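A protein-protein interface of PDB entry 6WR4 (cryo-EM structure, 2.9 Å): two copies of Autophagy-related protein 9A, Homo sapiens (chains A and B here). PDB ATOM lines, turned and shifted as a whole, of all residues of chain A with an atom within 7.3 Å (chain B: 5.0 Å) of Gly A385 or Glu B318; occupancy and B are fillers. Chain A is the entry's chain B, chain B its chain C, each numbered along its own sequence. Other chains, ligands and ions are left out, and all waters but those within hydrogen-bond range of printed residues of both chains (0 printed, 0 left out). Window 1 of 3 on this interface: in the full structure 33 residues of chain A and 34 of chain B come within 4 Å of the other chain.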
ATOM      1  N   GLY A 380      22.177  -5.927   3.070  1.00  0.00           N
ATOM      2  CA  GLY A 380      23.037  -6.871   3.762  1.00  0.00           C
ATOM      3  C   GLY A 380      24.260  -6.186   4.338  1.00  0.00           C
ATOM      4  O   GLY A 380      24.805  -6.616   5.354  1.00  0.00           O
ATOM      5  N   ALA A 381      24.707  -5.109   3.693  1.00  0.00           N
ATOM      6  CA  ALA A 381      25.828  -4.329   4.201  1.00  0.00           C
ATOM      7  C   ALA A 381      25.406  -3.425   5.351  1.00  0.00           C
ATOM      8  O   ALA A 381      26.250  -3.012   6.150  1.00  0.00           O
ATOM      9  CB  ALA A 381      26.444  -3.511   3.070  1.00  0.00           C
ATOM     10  N   PHE A 382      24.114  -3.093   5.447  1.00  0.00           N
ATOM     11  CA  PHE A 382      23.622  -2.356   6.609  1.00  0.00           C
ATOM     12  C   PHE A 382      23.632  -3.239   7.846  1.00  0.00           C
ATOM     13  O   PHE A 382      24.102  -2.830   8.910  1.00  0.00           O
ATOM     14  CB  PHE A 382      22.208  -1.815   6.360  1.00  0.00           C
ATOM     15  CG  PHE A 382      21.665  -0.976   7.502  1.00  0.00           C
ATOM     16  CD1 PHE A 382      22.039   0.348   7.636  1.00  0.00           C
ATOM     17  CD2 PHE A 382      20.803  -1.518   8.448  1.00  0.00           C
ATOM     18  CE1 PHE A 382      21.565   1.114   8.676  1.00  0.00           C
ATOM     19  CE2 PHE A 382      20.336  -0.757   9.501  1.00  0.00           C
ATOM     20  CZ  PHE A 382      20.714   0.560   9.607  1.00  0.00           C
ATOM     21  N   PHE A 383      23.088  -4.453   7.726  1.00  0.00           N
ATOM     22  CA  PHE A 383      22.936  -5.329   8.883  1.00  0.00           C
ATOM     23  C   PHE A 383      24.276  -5.840   9.389  1.00  0.00           C
ATOM     24  O   PHE A 383      24.410  -6.133  10.580  1.00  0.00           O
ATOM     25  CB  PHE A 383      22.025  -6.503   8.535  1.00  0.00           C
ATOM     26  CG  PHE A 383      20.580  -6.130   8.363  1.00  0.00           C
ATOM     27  CD1 PHE A 383      20.043  -5.020   8.989  1.00  0.00           C
ATOM     28  CD2 PHE A 383      19.768  -6.875   7.532  1.00  0.00           C
ATOM     29  CE1 PHE A 383      18.717  -4.689   8.807  1.00  0.00           C
ATOM     30  CE2 PHE A 383      18.446  -6.543   7.348  1.00  0.00           C
ATOM     31  CZ  PHE A 383      17.923  -5.450   7.985  1.00  0.00           C
ATOM     32  N   ALA A 384      25.274  -5.959   8.512  1.00  0.00           N
ATOM     33  CA  ALA A 384      26.592  -6.399   8.953  1.00  0.00           C
ATOM     34  C   ALA A 384      27.446  -5.222   9.401  1.00  0.00           C
ATOM     35  O   ALA A 384      28.276  -5.354  10.305  1.00  0.00           O
ATOM     36  CB  ALA A 384      27.286  -7.172   7.835  1.00  0.00           C
ATOM     37  N   GLY A 385      27.256  -4.056   8.781  1.00  0.00           N
ATOM     38  CA  GLY A 385      28.017  -2.882   9.182  1.00  0.00           C
ATOM     39  C   GLY A 385      27.544  -2.297  10.499  1.00  0.00           C
ATOM     40  O   GLY A 385      28.257  -1.529  11.145  1.00  0.00           O
ATOM     41  N   SER A 386      26.325  -2.644  10.907  1.00  0.00           N
ATOM     42  CA  SER A 386      25.778  -2.108  12.145  1.00  0.00           C
ATOM     43  C   SER A 386      26.305  -2.866  13.351  1.00  0.00           C
ATOM     44  O   SER A 386      26.473  -2.287  14.428  1.00  0.00           O
ATOM     45  CB  SER A 386      24.258  -2.169  12.101  1.00  0.00           C
ATOM     46  OG  SER A 386      23.774  -1.433  10.996  1.00  0.00           O
ATOM     47  N   ILE A 387      26.561  -4.165  13.193  1.00  0.00           N
ATOM     48  CA  ILE A 387      27.141  -4.959  14.271  1.00  0.00           C
ATOM     49  C   ILE A 387      28.670  -4.851  14.271  1.00  0.00           C
ATOM     50  O   ILE A 387      29.310  -5.021  15.315  1.00  0.00           O
ATOM     51  CB  ILE A 387      26.602  -6.405  14.167  1.00  0.00           C
ATOM     52  CG1 ILE A 387      27.183  -7.363  15.222  1.00  0.00           C
ATOM     53  CG2 ILE A 387      26.711  -6.920  12.767  1.00  0.00           C
ATOM     54  CD1 ILE A 387      26.827  -7.020  16.634  1.00  0.00           C
ATOM     55  N   LEU A 388      29.278  -4.511  13.129  1.00  0.00           N
ATOM     56  CA  LEU A 388      30.676  -4.079  13.141  1.00  0.00           C
ATOM     57  C   LEU A 388      30.861  -2.799  13.936  1.00  0.00           C
ATOM     58  O   LEU A 388      31.720  -2.732  14.822  1.00  0.00           O
ATOM     59  CB  LEU A 388      31.215  -3.863  11.729  1.00  0.00           C
ATOM     60  CG  LEU A 388      31.810  -5.022  10.959  1.00  0.00           C
ATOM     61  CD1 LEU A 388      32.217  -4.539   9.594  1.00  0.00           C
ATOM     62  CD2 LEU A 388      33.010  -5.506  11.727  1.00  0.00           C
ATOM     63  N   ALA A 389      30.066  -1.771  13.623  1.00  0.00           N
ATOM     64  CA  ALA A 389      30.232  -0.459  14.239  1.00  0.00           C
ATOM     65  C   ALA A 389      29.955  -0.489  15.731  1.00  0.00           C
ATOM     66  O   ALA A 389      30.497   0.331  16.473  1.00  0.00           O
ATOM     67  CB  ALA A 389      29.323   0.558  13.557  1.00  0.00           C
ATOM     68  N   VAL A 390      29.127  -1.424  16.192  1.00  0.00           N
ATOM     69  CA  VAL A 390      29.024  -1.655  17.626  1.00  0.00           C
ATOM     70  C   VAL A 390      30.308  -2.273  18.151  1.00  0.00           C
ATOM     71  O   VAL A 390      30.895  -1.775  19.114  1.00  0.00           O
ATOM     72  CB  VAL A 390      27.797  -2.522  17.946  1.00  0.00           C
ATOM     73  CG1 VAL A 390      27.820  -2.951  19.389  1.00  0.00           C
ATOM     74  CG2 VAL A 390      26.553  -1.730  17.685  1.00  0.00           C
ATOM     75  N   LEU A 391      30.790  -3.336  17.506  1.00  0.00           N
ATOM     76  CA  LEU A 391      32.011  -4.007  17.938  1.00  0.00           C
ATOM     77  C   LEU A 391      33.274  -3.190  17.712  1.00  0.00           C
ATOM     78  O   LEU A 391      34.208  -3.320  18.503  1.00  0.00           O
ATOM     79  CB  LEU A 391      32.165  -5.354  17.233  1.00  0.00           C
ATOM     80  CG  LEU A 391      31.213  -6.454  17.686  1.00  0.00           C
ATOM     81  CD1 LEU A 391      31.372  -7.679  16.815  1.00  0.00           C
ATOM     82  CD2 LEU A 391      31.475  -6.785  19.134  1.00  0.00           C
ATOM     83  N   ILE A 392      33.336  -2.372  16.658  1.00  0.00           N
ATOM     84  CA  ILE A 392      34.470  -1.465  16.480  1.00  0.00           C
ATOM     85  C   ILE A 392      34.519  -0.432  17.598  1.00  0.00           C
ATOM     86  O   ILE A 392      35.563  -0.237  18.229  1.00  0.00           O
ATOM     87  CB  ILE A 392      34.412  -0.793  15.095  1.00  0.00           C
ATOM     88  CG1 ILE A 392      34.806  -1.777  13.997  1.00  0.00           C
ATOM     89  CG2 ILE A 392      35.257   0.463  15.049  1.00  0.00           C
ATOM     90  CD1 ILE A 392      34.596  -1.231  12.613  1.00  0.00           C
ATOM     91  N   LEU A 414      32.694 -10.352   9.435  1.00  0.00           N
ATOM     92  CA  LEU A 414      31.779  -9.272   9.074  1.00  0.00           C
ATOM     93  C   LEU A 414      32.493  -8.197   8.277  1.00  0.00           C
ATOM     94  O   LEU A 414      31.867  -7.497   7.478  1.00  0.00           O
ATOM     95  CB  LEU A 414      31.137  -8.654  10.312  1.00  0.00           C
ATOM     96  CG  LEU A 414      30.146  -9.486  11.110  1.00  0.00           C
ATOM     97  CD1 LEU A 414      29.852  -8.752  12.375  1.00  0.00           C
ATOM     98  CD2 LEU A 414      28.885  -9.711  10.316  1.00  0.00           C
ATOM     99  N   GLY A 415      33.797  -8.043   8.492  1.00  0.00           N
ATOM    100  CA  GLY A 415      34.552  -7.081   7.712  1.00  0.00           C
ATOM    101  C   GLY A 415      34.698  -7.493   6.262  1.00  0.00           C
ATOM    102  O   GLY A 415      34.777  -6.647   5.372  1.00  0.00           O
ATOM    103  N   THR A 417      32.389  -9.554   4.905  1.00  0.00           N
ATOM    104  CA  THR A 417      31.004  -9.534   4.439  1.00  0.00           C
ATOM    105  C   THR A 417      30.624  -8.154   3.921  1.00  0.00           C
ATOM    106  O   THR A 417      30.009  -8.026   2.857  1.00  0.00           O
ATOM    107  CB  THR A 417      30.063  -9.953   5.567  1.00  0.00           C
ATOM    108  OG1 THR A 417      30.451 -11.239   6.056  1.00  0.00           O
ATOM    109  CG2 THR A 417      28.630 -10.032   5.074  1.00  0.00           C
ATOM    110  N   VAL A 418      30.998  -7.110   4.661  1.00  0.00           N
ATOM    111  CA  VAL A 418      30.804  -5.734   4.220  1.00  0.00           C
ATOM    112  C   VAL A 418      31.641  -5.434   2.983  1.00  0.00           C
ATOM    113  O   VAL A 418      31.193  -4.718   2.078  1.00  0.00           O
ATOM    114  CB  VAL A 418      31.121  -4.790   5.399  1.00  0.00           C
ATOM    115  CG1 VAL A 418      31.166  -3.346   4.978  1.00  0.00           C
ATOM    116  CG2 VAL A 418      30.083  -4.959   6.479  1.00  0.00           C
ATOM    117  N   THR A 419      32.833  -6.026   2.890  1.00  0.00           N
ATOM    118  CA  THR A 419      33.716  -5.754   1.761  1.00  0.00           C
ATOM    119  C   THR A 419      33.204  -6.415   0.483  1.00  0.00           C
ATOM    120  O   THR A 419      33.346  -5.854  -0.610  1.00  0.00           O
ATOM    121  CB  THR A 419      35.129  -6.227   2.101  1.00  0.00           C
ATOM    122  OG1 THR A 419      35.499  -5.700   3.376  1.00  0.00           O
ATOM    123  CG2 THR A 419      36.134  -5.716   1.093  1.00  0.00           C
ATOM    124  N   ARG A 422      29.984  -4.192  -0.571  1.00  0.00           N
ATOM    125  CA  ARG A 422      30.386  -2.944  -1.220  1.00  0.00           C
ATOM    126  C   ARG A 422      30.872  -3.148  -2.648  1.00  0.00           C
ATOM    127  O   ARG A 422      30.865  -2.198  -3.437  1.00  0.00           O
ATOM    128  CB  ARG A 422      31.492  -2.236  -0.437  1.00  0.00           C
ATOM    129  CG  ARG A 422      31.100  -1.124   0.530  1.00  0.00           C
ATOM    130  CD  ARG A 422      30.375  -1.538   1.771  1.00  0.00           C
ATOM    131  NE  ARG A 422      30.390  -0.414   2.718  1.00  0.00           N
ATOM    132  CZ  ARG A 422      29.511  -0.223   3.696  1.00  0.00           C
ATOM    133  NH1 ARG A 422      28.527  -1.078   3.891  1.00  0.00           N
ATOM    134  NH2 ARG A 422      29.630   0.822   4.489  1.00  0.00           N
ATOM    135  N   PHE B 314      24.755   3.478  13.159  1.00  0.00           N
ATOM    136  CA  PHE B 314      24.641   2.133  12.611  1.00  0.00           C
ATOM    137  C   PHE B 314      24.974   2.099  11.130  1.00  0.00           C
ATOM    138  O   PHE B 314      25.015   1.023  10.525  1.00  0.00           O
ATOM    139  CB  PHE B 314      23.236   1.591  12.854  1.00  0.00           C
ATOM    140  CG  PHE B 314      22.997   1.147  14.259  1.00  0.00           C
ATOM    141  CD1 PHE B 314      24.046   0.790  15.073  1.00  0.00           C
ATOM    142  CD2 PHE B 314      21.721   1.114  14.774  1.00  0.00           C
ATOM    143  CE1 PHE B 314      23.821   0.383  16.368  1.00  0.00           C
ATOM    144  CE2 PHE B 314      21.491   0.715  16.070  1.00  0.00           C
ATOM    145  CZ  PHE B 314      22.539   0.351  16.864  1.00  0.00           C
ATOM    146  N   TYR B 316      27.328   4.693   9.598  1.00  0.00           N
ATOM    147  CA  TYR B 316      28.498   5.482   9.241  1.00  0.00           C
ATOM    148  C   TYR B 316      29.683   5.312  10.181  1.00  0.00           C
ATOM    149  O   TYR B 316      30.768   5.802   9.862  1.00  0.00           O
ATOM    150  CB  TYR B 316      28.137   6.974   9.160  1.00  0.00           C
ATOM    151  CG  TYR B 316      27.123   7.282   8.091  1.00  0.00           C
ATOM    152  CD1 TYR B 316      27.477   7.276   6.750  1.00  0.00           C
ATOM    153  CD2 TYR B 316      25.808   7.579   8.422  1.00  0.00           C
ATOM    154  CE1 TYR B 316      26.546   7.546   5.765  1.00  0.00           C
ATOM    155  CE2 TYR B 316      24.869   7.851   7.445  1.00  0.00           C
ATOM    156  CZ  TYR B 316      25.246   7.838   6.119  1.00  0.00           C
ATOM    157  OH  TYR B 316      24.318   8.110   5.146  1.00  0.00           O
ATOM    158  N   ALA B 317      29.517   4.640  11.320  1.00  0.00           N
ATOM    159  CA  ALA B 317      30.581   4.626  12.319  1.00  0.00           C
ATOM    160  C   ALA B 317      31.655   3.599  11.989  1.00  0.00           C
ATOM    161  O   ALA B 317      32.773   3.671  12.507  1.00  0.00           O
ATOM    162  CB  ALA B 317      30.007   4.360  13.704  1.00  0.00           C
ATOM    163  N   GLU B 318      31.335   2.617  11.150  1.00  0.00           N
ATOM    164  CA  GLU B 318      32.361   1.662  10.746  1.00  0.00           C
ATOM    165  C   GLU B 318      33.082   2.165   9.502  1.00  0.00           C
ATOM    166  O   GLU B 318      34.206   1.745   9.211  1.00  0.00           O
ATOM    167  CB  GLU B 318      31.723   0.262  10.608  1.00  0.00           C
ATOM    168  CG  GLU B 318      32.303  -0.890   9.716  1.00  0.00           C
ATOM    169  CD  GLU B 318      32.405  -0.664   8.218  1.00  0.00           C
ATOM    170  OE1 GLU B 318      31.659   0.175   7.679  1.00  0.00           O
ATOM    171  OE2 GLU B 318      33.251  -1.325   7.583  1.00  0.00           O
ATOM    172  N   VAL B 319      32.447   3.072   8.760  1.00  0.00           N
ATOM    173  CA  VAL B 319      33.075   3.670   7.586  1.00  0.00           C
ATOM    174  C   VAL B 319      34.132   4.682   8.020  1.00  0.00           C
ATOM    175  O   VAL B 319      35.073   4.987   7.279  1.00  0.00           O
ATOM    176  CB  VAL B 319      31.990   4.298   6.689  1.00  0.00           C
ATOM    177  CG1 VAL B 319      32.538   4.841   5.371  1.00  0.00           C
ATOM    178  CG2 VAL B 319      30.901   3.286   6.429  1.00  0.00           C
ATOM    179  N   LEU B 320      34.013   5.187   9.253  1.00  0.00           N
ATOM    180  CA  LEU B 320      35.042   6.060   9.813  1.00  0.00           C
ATOM    181  C   LEU B 320      36.365   5.332  10.001  1.00  0.00           C
ATOM    182  O   LEU B 320      37.428   5.900   9.734  1.00  0.00           O
ATOM    183  CB  LEU B 320      34.581   6.642  11.147  1.00  0.00           C
ATOM    184  CG  LEU B 320      33.580   7.786  11.105  1.00  0.00           C
ATOM    185  CD1 LEU B 320      33.101   8.117  12.502  1.00  0.00           C
ATOM    186  CD2 LEU B 320      34.269   8.981  10.493  1.00  0.00           C
ATOM    187  N   LYS B 321      36.325   4.078  10.456  1.00  0.00           N
ATOM    188  CA  LYS B 321      37.569   3.362  10.706  1.00  0.00           C
ATOM    189  C   LYS B 321      38.247   2.944   9.406  1.00  0.00           C
ATOM    190  O   LYS B 321      39.457   3.140   9.244  1.00  0.00           O
ATOM    191  CB  LYS B 321      37.323   2.148  11.596  1.00  0.00           C
ATOM    192  CG  LYS B 321      38.610   1.452  12.007  1.00  0.00           C
ATOM    193  CD  LYS B 321      38.360   0.337  12.993  1.00  0.00           C
ATOM    194  CE  LYS B 321      39.644  -0.361  13.377  1.00  0.00           C
ATOM    195  NZ  LYS B 321      39.416  -1.467  14.352  1.00  0.00           N
ATOM    196  N   ARG B 322      37.495   2.353   8.478  1.00  0.00           N
ATOM    197  CA  ARG B 322      38.059   1.988   7.184  1.00  0.00           C
ATOM    198  C   ARG B 322      38.463   3.185   6.337  1.00  0.00           C
ATOM    199  O   ARG B 322      39.649   3.387   6.061  1.00  0.00           O
ATOM    200  CB  ARG B 322      37.081   1.160   6.362  1.00  0.00           C
ATOM    201  CG  ARG B 322      36.828  -0.233   6.847  1.00  0.00           C
ATOM    202  CD  ARG B 322      36.009  -0.968   5.808  1.00  0.00           C
ATOM    203  NE  ARG B 322      34.666  -0.412   5.669  1.00  0.00           N
ATOM    204  CZ  ARG B 322      34.227   0.226   4.588  1.00  0.00           C
ATOM    205  NH1 ARG B 322      32.991   0.699   4.551  1.00  0.00           N
ATOM    206  NH2 ARG B 322      35.029   0.399   3.547  1.00  0.00           N
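The side-chain hydroxyl of Ser A386 sits at hydrogen-bond distance from the backbone carbonyl oxygen of Phe B314, at 2.8 Å.
The guanidinium group (NH2) of Arg A422 lies close to the guanidinium group (NH1) of Arg B322, 3.4 Å away.
The guanidinium group of Arg A422 lies within salt-bridge range of the side-chain carboxylate of Glu B318 (3.8 Å).
OE2 of Glu B318 is in salt-bridge range of NE of Arg B322, 2.5 Å away.
The backbone carbonyl oxygen of Phe A382 sits at hydrogen-bond distance from the side-chain hydroxyl of Ser A386 (2.5 Å).
Among the printed residues, pairs that only touch across the chains: Arg A422 with Val B319 (3.4 Å), Leu A388 with Glu B318 (3.7 Å), Val A390 with Phe B314 (3.7 Å), Ile A392 with Glu B318 (3.7 Å), Ile A392 with Lys B321 (3.7 Å), Ala A389 with Glu B318 (3.8 Å), Ala A389 with Ala B317 (3.9 Å), Val A418 with Glu B318 (3.9 Å), Phe A382 with Phe B314 (3.9 Å) and Gly A385 with Glu B318 (3.9 Å).
Gly A385 touches one residue of chain B.
Ile A387 touches none of the printed residues of chain B.
Of the printed residues of chain B, Ile A392 touches Glu B318 and Lys B321.
Thr A417 touches none of the printed residues of chain B.
Glu B318 touches just these residues of chain A: Gly A385, Leu A388, Ala A389, Ile A392, Val A418 and Arg A422.
Of the printed residues of chain A, Lys B321 touches Ile A392 (3.7 Å).
The nearest printed residue of chain A that does not touch Ala B317 is Ile A392 (4.8 Å).
Of the 8 printed residues of chain B, 6 touch a printed residue of chain A.
Along chain B the printed residues that touch a printed residue of chain A span positions 314 to 322.
Printed residues of chain A that touch a printed residue of chain B: Phe A382, Gly A385, Ser A386, Leu A388, Ala A389, Val A390, Ile A392, Val A418 and Arg A422.
Hydrophobic or aromatic side chains of chain A that line the printed part of chain B: Phe A382, Leu A388, Ala A389, Val A390, Ile A392 and Val A418.
Among the printed residues, Asp or Glu carboxylates within 4 Å of a Lys or Arg side-chain nitrogen of the other chain: Arg A422 with Glu B318 (3.8 Å).
No position is printed for both chains.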
